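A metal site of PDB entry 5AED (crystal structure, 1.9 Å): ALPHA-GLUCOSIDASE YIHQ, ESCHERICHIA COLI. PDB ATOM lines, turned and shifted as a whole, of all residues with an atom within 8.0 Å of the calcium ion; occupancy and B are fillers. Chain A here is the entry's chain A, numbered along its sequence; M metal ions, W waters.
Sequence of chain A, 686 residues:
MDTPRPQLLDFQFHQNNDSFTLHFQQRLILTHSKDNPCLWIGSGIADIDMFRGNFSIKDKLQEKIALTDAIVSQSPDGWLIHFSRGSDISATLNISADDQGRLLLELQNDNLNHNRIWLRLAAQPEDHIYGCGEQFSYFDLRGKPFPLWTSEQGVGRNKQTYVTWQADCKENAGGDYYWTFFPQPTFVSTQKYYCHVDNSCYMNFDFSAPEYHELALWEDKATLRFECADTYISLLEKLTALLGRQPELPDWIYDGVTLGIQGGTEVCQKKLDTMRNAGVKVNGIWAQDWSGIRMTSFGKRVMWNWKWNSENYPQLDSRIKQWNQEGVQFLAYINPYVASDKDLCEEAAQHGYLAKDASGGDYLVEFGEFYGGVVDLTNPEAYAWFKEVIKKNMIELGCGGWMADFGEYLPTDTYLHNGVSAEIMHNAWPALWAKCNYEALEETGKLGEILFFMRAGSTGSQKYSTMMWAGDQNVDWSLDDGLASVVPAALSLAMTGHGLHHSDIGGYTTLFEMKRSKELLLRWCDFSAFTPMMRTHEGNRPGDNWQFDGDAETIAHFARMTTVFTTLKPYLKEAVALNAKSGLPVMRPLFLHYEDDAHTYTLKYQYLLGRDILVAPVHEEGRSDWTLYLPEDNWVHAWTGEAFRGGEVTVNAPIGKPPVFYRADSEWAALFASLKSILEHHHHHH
The calcium ion is bound by the side-chain amide oxygen (OE1) of Gln 153 (2.3 Å).
Water W1 is bound to the calcium ion, at 2.3 Å.
The calcium ion is bound by the backbone carbonyl oxygen (O) of Gly 154, at 2.4 Å.
The calcium ion is bound by O of Asp 472 (2.4 Å).
OD2 of Asp 481 binds the calcium ion, at 2.5 Å.
The side-chain carboxylate (OD2) of Asp 472 is bound to the calcium ion (2.5 Å).
The calcium ion is bound by OD1 of Asp 481 (2.6 Å).
The calcium ion has seven donor atoms within binding distance.
The backbone carbonyl oxygen of Gln 153 lies within hydrogen-bond range of the guanidinium group of Arg 157 (3.0 Å).
The backbone NH (N) of Asn 474 lies within hydrogen-bond range of the backbone carbonyl oxygen (O) of Asp 481 (2.8 Å).
The side-chain carboxylate (OD2) of Asp 481 lies close to the backbone NH (N) of Gly 156 (2.9 Å).
Water W1 lies within hydrogen-bond range of OD1 of Asn 474 (2.7 Å) and OG1 of Thr 509 (2.8 Å).
Within 4 Å of the calcium ion: Gln 153, Gly 154, Asp 472 and Asp 481.
The nearest printed residue that does not touch the calcium ion is Val 155 (4.3 Å).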
ATOM      1  N   PHE A 136      -1.868  24.961 -22.741  1.00  0.00           N
ATOM      2  CA  PHE A 136      -1.544  24.088 -21.638  1.00  0.00           C
ATOM      3  C   PHE A 136      -0.442  24.615 -20.723  1.00  0.00           C
ATOM      4  O   PHE A 136      -0.351  24.189 -19.543  1.00  0.00           O
ATOM      5  CB  PHE A 136      -1.125  22.719 -22.220  1.00  0.00           C
ATOM      6  CG  PHE A 136      -2.259  21.953 -22.816  1.00  0.00           C
ATOM      7  CD1 PHE A 136      -3.002  21.071 -22.043  1.00  0.00           C
ATOM      8  CD2 PHE A 136      -2.566  22.055 -24.152  1.00  0.00           C
ATOM      9  CE1 PHE A 136      -4.053  20.331 -22.610  1.00  0.00           C
ATOM     10  CE2 PHE A 136      -3.629  21.339 -24.701  1.00  0.00           C
ATOM     11  CZ  PHE A 136      -4.389  20.505 -23.930  1.00  0.00           C
ATOM     12  N   GLU A 152       0.422  17.645 -32.937  1.00  0.00           N
ATOM     13  CA  GLU A 152       0.617  16.975 -31.651  1.00  0.00           C
ATOM     14  C   GLU A 152       0.997  17.964 -30.559  1.00  0.00           C
ATOM     15  O   GLU A 152       1.616  19.021 -30.821  1.00  0.00           O
ATOM     16  CB  GLU A 152       1.605  15.785 -31.714  1.00  0.00           C
ATOM     17  CG  GLU A 152       1.240  14.699 -32.706  1.00  0.00           C
ATOM     18  CD  GLU A 152      -0.245  14.294 -32.778  1.00  0.00           C
ATOM     19  OE1 GLU A 152      -0.909  14.052 -31.738  1.00  0.00           O
ATOM     20  OE2 GLU A 152      -0.768  14.257 -33.910  1.00  0.00           O
ATOM     21  N   GLN A 153       0.561  17.622 -29.340  1.00  0.00           N
ATOM     22  CA  GLN A 153       0.552  18.504 -28.206  1.00  0.00           C
ATOM     23  C   GLN A 153       1.932  18.463 -27.481  1.00  0.00           C
ATOM     24  O   GLN A 153       2.297  19.414 -26.798  1.00  0.00           O
ATOM     25  CB  GLN A 153      -0.628  18.072 -27.292  1.00  0.00           C
ATOM     26  CG  GLN A 153      -0.939  18.997 -26.124  1.00  0.00           C
ATOM     27  CD  GLN A 153      -0.554  18.395 -24.781  1.00  0.00           C
ATOM     28  OE1 GLN A 153       0.124  17.367 -24.696  1.00  0.00           O
ATOM     29  NE2 GLN A 153      -1.003  19.005 -23.754  1.00  0.00           N
ATOM     30  N   GLY A 154       2.686  17.378 -27.664  1.00  0.00           N
ATOM     31  CA  GLY A 154       4.020  17.251 -27.042  1.00  0.00           C
ATOM     32  C   GLY A 154       4.000  16.278 -25.890  1.00  0.00           C
ATOM     33  O   GLY A 154       2.957  16.030 -25.286  1.00  0.00           O
ATOM     34  N   VAL A 155       5.140  15.726 -25.599  1.00  0.00           N
ATOM     35  CA  VAL A 155       5.334  14.800 -24.482  1.00  0.00           C
ATOM     36  C   VAL A 155       6.428  15.458 -23.639  1.00  0.00           C
ATOM     37  O   VAL A 155       7.633  15.421 -24.076  1.00  0.00           O
ATOM     38  CB  VAL A 155       5.787  13.414 -24.977  1.00  0.00           C
ATOM     39  CG1 VAL A 155       6.099  12.523 -23.801  1.00  0.00           C
ATOM     40  CG2 VAL A 155       4.719  12.749 -25.833  1.00  0.00           C
ATOM     41  N   GLY A 156       6.042  16.030 -22.502  1.00  0.00           N
ATOM     42  CA  GLY A 156       6.936  16.801 -21.597  1.00  0.00           C
ATOM     43  C   GLY A 156       6.704  18.312 -21.803  1.00  0.00           C
ATOM     44  O   GLY A 156       6.470  19.073 -20.851  1.00  0.00           O
ATOM     45  N   ARG A 157       6.783  18.744 -23.077  1.00  0.00           N
ATOM     46  CA  ARG A 157       6.456  20.124 -23.496  1.00  0.00           C
ATOM     47  C   ARG A 157       7.403  21.219 -22.901  1.00  0.00           C
ATOM     48  O   ARG A 157       7.019  22.370 -22.889  1.00  0.00           O
ATOM     49  CB  ARG A 157       4.998  20.460 -23.237  1.00  0.00           C
ATOM     50  CG  ARG A 157       4.006  19.424 -23.735  1.00  0.00           C
ATOM     51  CD  ARG A 157       2.585  19.830 -23.581  1.00  0.00           C
ATOM     52  NE  ARG A 157       2.196  21.044 -24.291  1.00  0.00           N
ATOM     53  CZ  ARG A 157       2.112  22.240 -23.740  1.00  0.00           C
ATOM     54  NH1 ARG A 157       2.324  22.398 -22.469  1.00  0.00           N
ATOM     55  NH2 ARG A 157       1.796  23.264 -24.493  1.00  0.00           N
ATOM     56  N   ALA A 173       9.267  14.908 -30.648  1.00  0.00           N
ATOM     57  CA  ALA A 173       7.926  14.726 -30.039  1.00  0.00           C
ATOM     58  C   ALA A 173       7.750  15.400 -28.661  1.00  0.00           C
ATOM     59  O   ALA A 173       6.632  15.373 -28.063  1.00  0.00           O
ATOM     60  CB  ALA A 173       7.576  13.217 -29.952  1.00  0.00           C
ATOM     61  N   GLY A 174       8.823  16.007 -28.169  1.00  0.00           N
ATOM     62  CA  GLY A 174       8.838  16.685 -26.905  1.00  0.00           C
ATOM     63  C   GLY A 174       7.923  17.904 -26.867  1.00  0.00           C
ATOM     64  O   GLY A 174       7.280  18.184 -25.871  1.00  0.00           O
ATOM     65  N   PHE A 181      -3.182  20.774 -30.053  1.00  0.00           N
ATOM     66  CA  PHE A 181      -4.120  20.288 -31.052  1.00  0.00           C
ATOM     67  C   PHE A 181      -5.364  21.143 -31.290  1.00  0.00           C
ATOM     68  O   PHE A 181      -6.178  20.846 -32.188  1.00  0.00           O
ATOM     69  CB  PHE A 181      -4.569  18.821 -30.745  1.00  0.00           C
ATOM     70  CG  PHE A 181      -4.680  18.485 -29.296  1.00  0.00           C
ATOM     71  CD1 PHE A 181      -5.532  19.187 -28.467  1.00  0.00           C
ATOM     72  CD2 PHE A 181      -3.883  17.513 -28.734  1.00  0.00           C
ATOM     73  CE1 PHE A 181      -5.616  18.903 -27.100  1.00  0.00           C
ATOM     74  CE2 PHE A 181      -3.983  17.196 -27.372  1.00  0.00           C
ATOM     75  CZ  PHE A 181      -4.803  17.924 -26.540  1.00  0.00           C
ATOM     76  N   ALA A 470      -8.863  16.959 -22.713  1.00  0.00           N
ATOM     77  CA  ALA A 470      -7.541  17.607 -22.751  1.00  0.00           C
ATOM     78  C   ALA A 470      -6.439  16.790 -23.385  1.00  0.00           C
ATOM     79  O   ALA A 470      -5.282  17.134 -23.236  1.00  0.00           O
ATOM     80  CB  ALA A 470      -7.131  17.999 -21.339  1.00  0.00           C
ATOM     81  N   GLY A 471      -6.775  15.680 -24.045  1.00  0.00           N
ATOM     82  CA  GLY A 471      -5.810  14.912 -24.768  1.00  0.00           C
ATOM     83  C   GLY A 471      -4.840  14.251 -23.848  1.00  0.00           C
ATOM     84  O   GLY A 471      -5.159  13.884 -22.730  1.00  0.00           O
ATOM     85  N   ASP A 472      -3.642  14.061 -24.391  1.00  0.00           N
ATOM     86  CA  ASP A 472      -2.641  13.215 -23.772  1.00  0.00           C
ATOM     87  C   ASP A 472      -1.843  13.989 -22.706  1.00  0.00           C
ATOM     88  O   ASP A 472      -1.004  14.770 -23.085  1.00  0.00           O
ATOM     89  CB  ASP A 472      -1.640  12.687 -24.864  1.00  0.00           C
ATOM     90  CG  ASP A 472      -1.083  13.842 -25.866  1.00  0.00           C
ATOM     91  OD1 ASP A 472      -1.940  14.301 -26.758  1.00  0.00           O
ATOM     92  OD2 ASP A 472       0.231  14.235 -25.720  1.00  0.00           O
ATOM     93  N   GLN A 473      -2.092  13.768 -21.408  1.00  0.00           N
ATOM     94  CA  GLN A 473      -1.139  14.172 -20.407  1.00  0.00           C
ATOM     95  C   GLN A 473      -0.237  13.032 -20.137  1.00  0.00           C
ATOM     96  O   GLN A 473      -0.617  11.869 -20.274  1.00  0.00           O
ATOM     97  CB  GLN A 473      -1.777  14.568 -19.062  1.00  0.00           C
ATOM     98  CG  GLN A 473      -2.361  15.956 -19.039  1.00  0.00           C
ATOM     99  CD  GLN A 473      -3.605  16.001 -19.867  1.00  0.00           C
ATOM    100  OE1 GLN A 473      -4.562  15.297 -19.580  1.00  0.00           O
ATOM    101  NE2 GLN A 473      -3.567  16.761 -20.961  1.00  0.00           N
ATOM    102  N   ASN A 474       0.971  13.357 -19.717  1.00  0.00           N
ATOM    103  CA  ASN A 474       1.856  12.375 -19.084  1.00  0.00           C
ATOM    104  C   ASN A 474       1.274  11.909 -17.766  1.00  0.00           C
ATOM    105  O   ASN A 474       0.563  12.679 -17.060  1.00  0.00           O
ATOM    106  CB  ASN A 474       3.226  13.024 -18.714  1.00  0.00           C
ATOM    107  CG  ASN A 474       4.054  13.367 -19.908  1.00  0.00           C
ATOM    108  OD1 ASN A 474       3.737  13.010 -21.026  1.00  0.00           O
ATOM    109  ND2 ASN A 474       5.177  14.046 -19.659  1.00  0.00           N
ATOM    110  N   ASP A 480       3.900  21.302 -17.184  1.00  0.00           N
ATOM    111  CA  ASP A 480       3.630  21.547 -18.562  1.00  0.00           C
ATOM    112  C   ASP A 480       2.933  20.387 -19.240  1.00  0.00           C
ATOM    113  O   ASP A 480       2.346  20.591 -20.298  1.00  0.00           O
ATOM    114  CB  ASP A 480       4.949  21.874 -19.283  1.00  0.00           C
ATOM    115  CG  ASP A 480       5.506  23.215 -18.817  1.00  0.00           C
ATOM    116  OD1 ASP A 480       4.935  24.221 -19.224  1.00  0.00           O
ATOM    117  OD2 ASP A 480       6.442  23.262 -18.031  1.00  0.00           O
ATOM    118  N   ASP A 481       3.014  19.197 -18.676  1.00  0.00           N
ATOM    119  CA  ASP A 481       2.259  18.062 -19.248  1.00  0.00           C
ATOM    120  C   ASP A 481       1.633  17.094 -18.276  1.00  0.00           C
ATOM    121  O   ASP A 481       1.237  15.987 -18.688  1.00  0.00           O
ATOM    122  CB  ASP A 481       3.187  17.264 -20.189  1.00  0.00           C
ATOM    123  CG  ASP A 481       2.501  16.693 -21.409  1.00  0.00           C
ATOM    124  OD1 ASP A 481       1.318  16.945 -21.620  1.00  0.00           O
ATOM    125  OD2 ASP A 481       3.187  15.988 -22.259  1.00  0.00           O
ATOM    126  N   GLY A 482       1.528  17.500 -17.025  1.00  0.00           N
ATOM    127  CA  GLY A 482       0.947  16.699 -15.945  1.00  0.00           C
ATOM    128  C   GLY A 482      -0.461  17.082 -15.643  1.00  0.00           C
ATOM    129  O   GLY A 482      -1.119  17.811 -16.407  1.00  0.00           O
ATOM    130  N   SER A 485      -1.520  20.875 -15.967  1.00  0.00           N
ATOM    131  CA  SER A 485      -1.683  21.463 -17.298  1.00  0.00           C
ATOM    132  C   SER A 485      -3.125  21.468 -17.798  1.00  0.00           C
ATOM    133  O   SER A 485      -3.475  22.228 -18.737  1.00  0.00           O
ATOM    134  CB  SER A 485      -0.806  20.742 -18.348  1.00  0.00           C
ATOM    135  OG  SER A 485      -1.241  19.404 -18.692  1.00  0.00           O
ATOM    136  N   TYR A 508      -2.416   9.819 -19.309  1.00  0.00           N
ATOM    137  CA  TYR A 508      -2.360   8.880 -20.426  1.00  0.00           C
ATOM    138  C   TYR A 508      -0.956   8.384 -20.826  1.00  0.00           C
ATOM    139  O   TYR A 508      -0.676   7.177 -20.815  1.00  0.00           O
ATOM    140  CB  TYR A 508      -3.010   9.564 -21.638  1.00  0.00           C
ATOM    141  CG  TYR A 508      -2.847   8.805 -22.895  1.00  0.00           C
ATOM    142  CD1 TYR A 508      -3.628   7.674 -23.147  1.00  0.00           C
ATOM    143  CD2 TYR A 508      -1.900   9.201 -23.863  1.00  0.00           C
ATOM    144  CE1 TYR A 508      -3.461   6.948 -24.323  1.00  0.00           C
ATOM    145  CE2 TYR A 508      -1.736   8.498 -25.046  1.00  0.00           C
ATOM    146  CZ  TYR A 508      -2.524   7.349 -25.261  1.00  0.00           C
ATOM    147  OH  TYR A 508      -2.414   6.616 -26.449  1.00  0.00           O
ATOM    148  N   THR A 509      -0.097   9.308 -21.201  1.00  0.00           N
ATOM    149  CA  THR A 509       1.195   8.966 -21.797  1.00  0.00           C
ATOM    150  C   THR A 509       2.163   8.291 -20.791  1.00  0.00           C
ATOM    151  O   THR A 509       2.602   8.856 -19.829  1.00  0.00           O
ATOM    152  CB  THR A 509       1.893  10.190 -22.439  1.00  0.00           C
ATOM    153  OG1 THR A 509       1.018  10.872 -23.346  1.00  0.00           O
ATOM    154  CG2 THR A 509       3.127   9.698 -23.247  1.00  0.00           C
HETATM  155 CA    CA M   1       1.194  15.560 -23.774  1.00  0.00          CA
HETATM  156  O   HOH W   1       2.010  13.509 -23.027  1.00  0.00           O
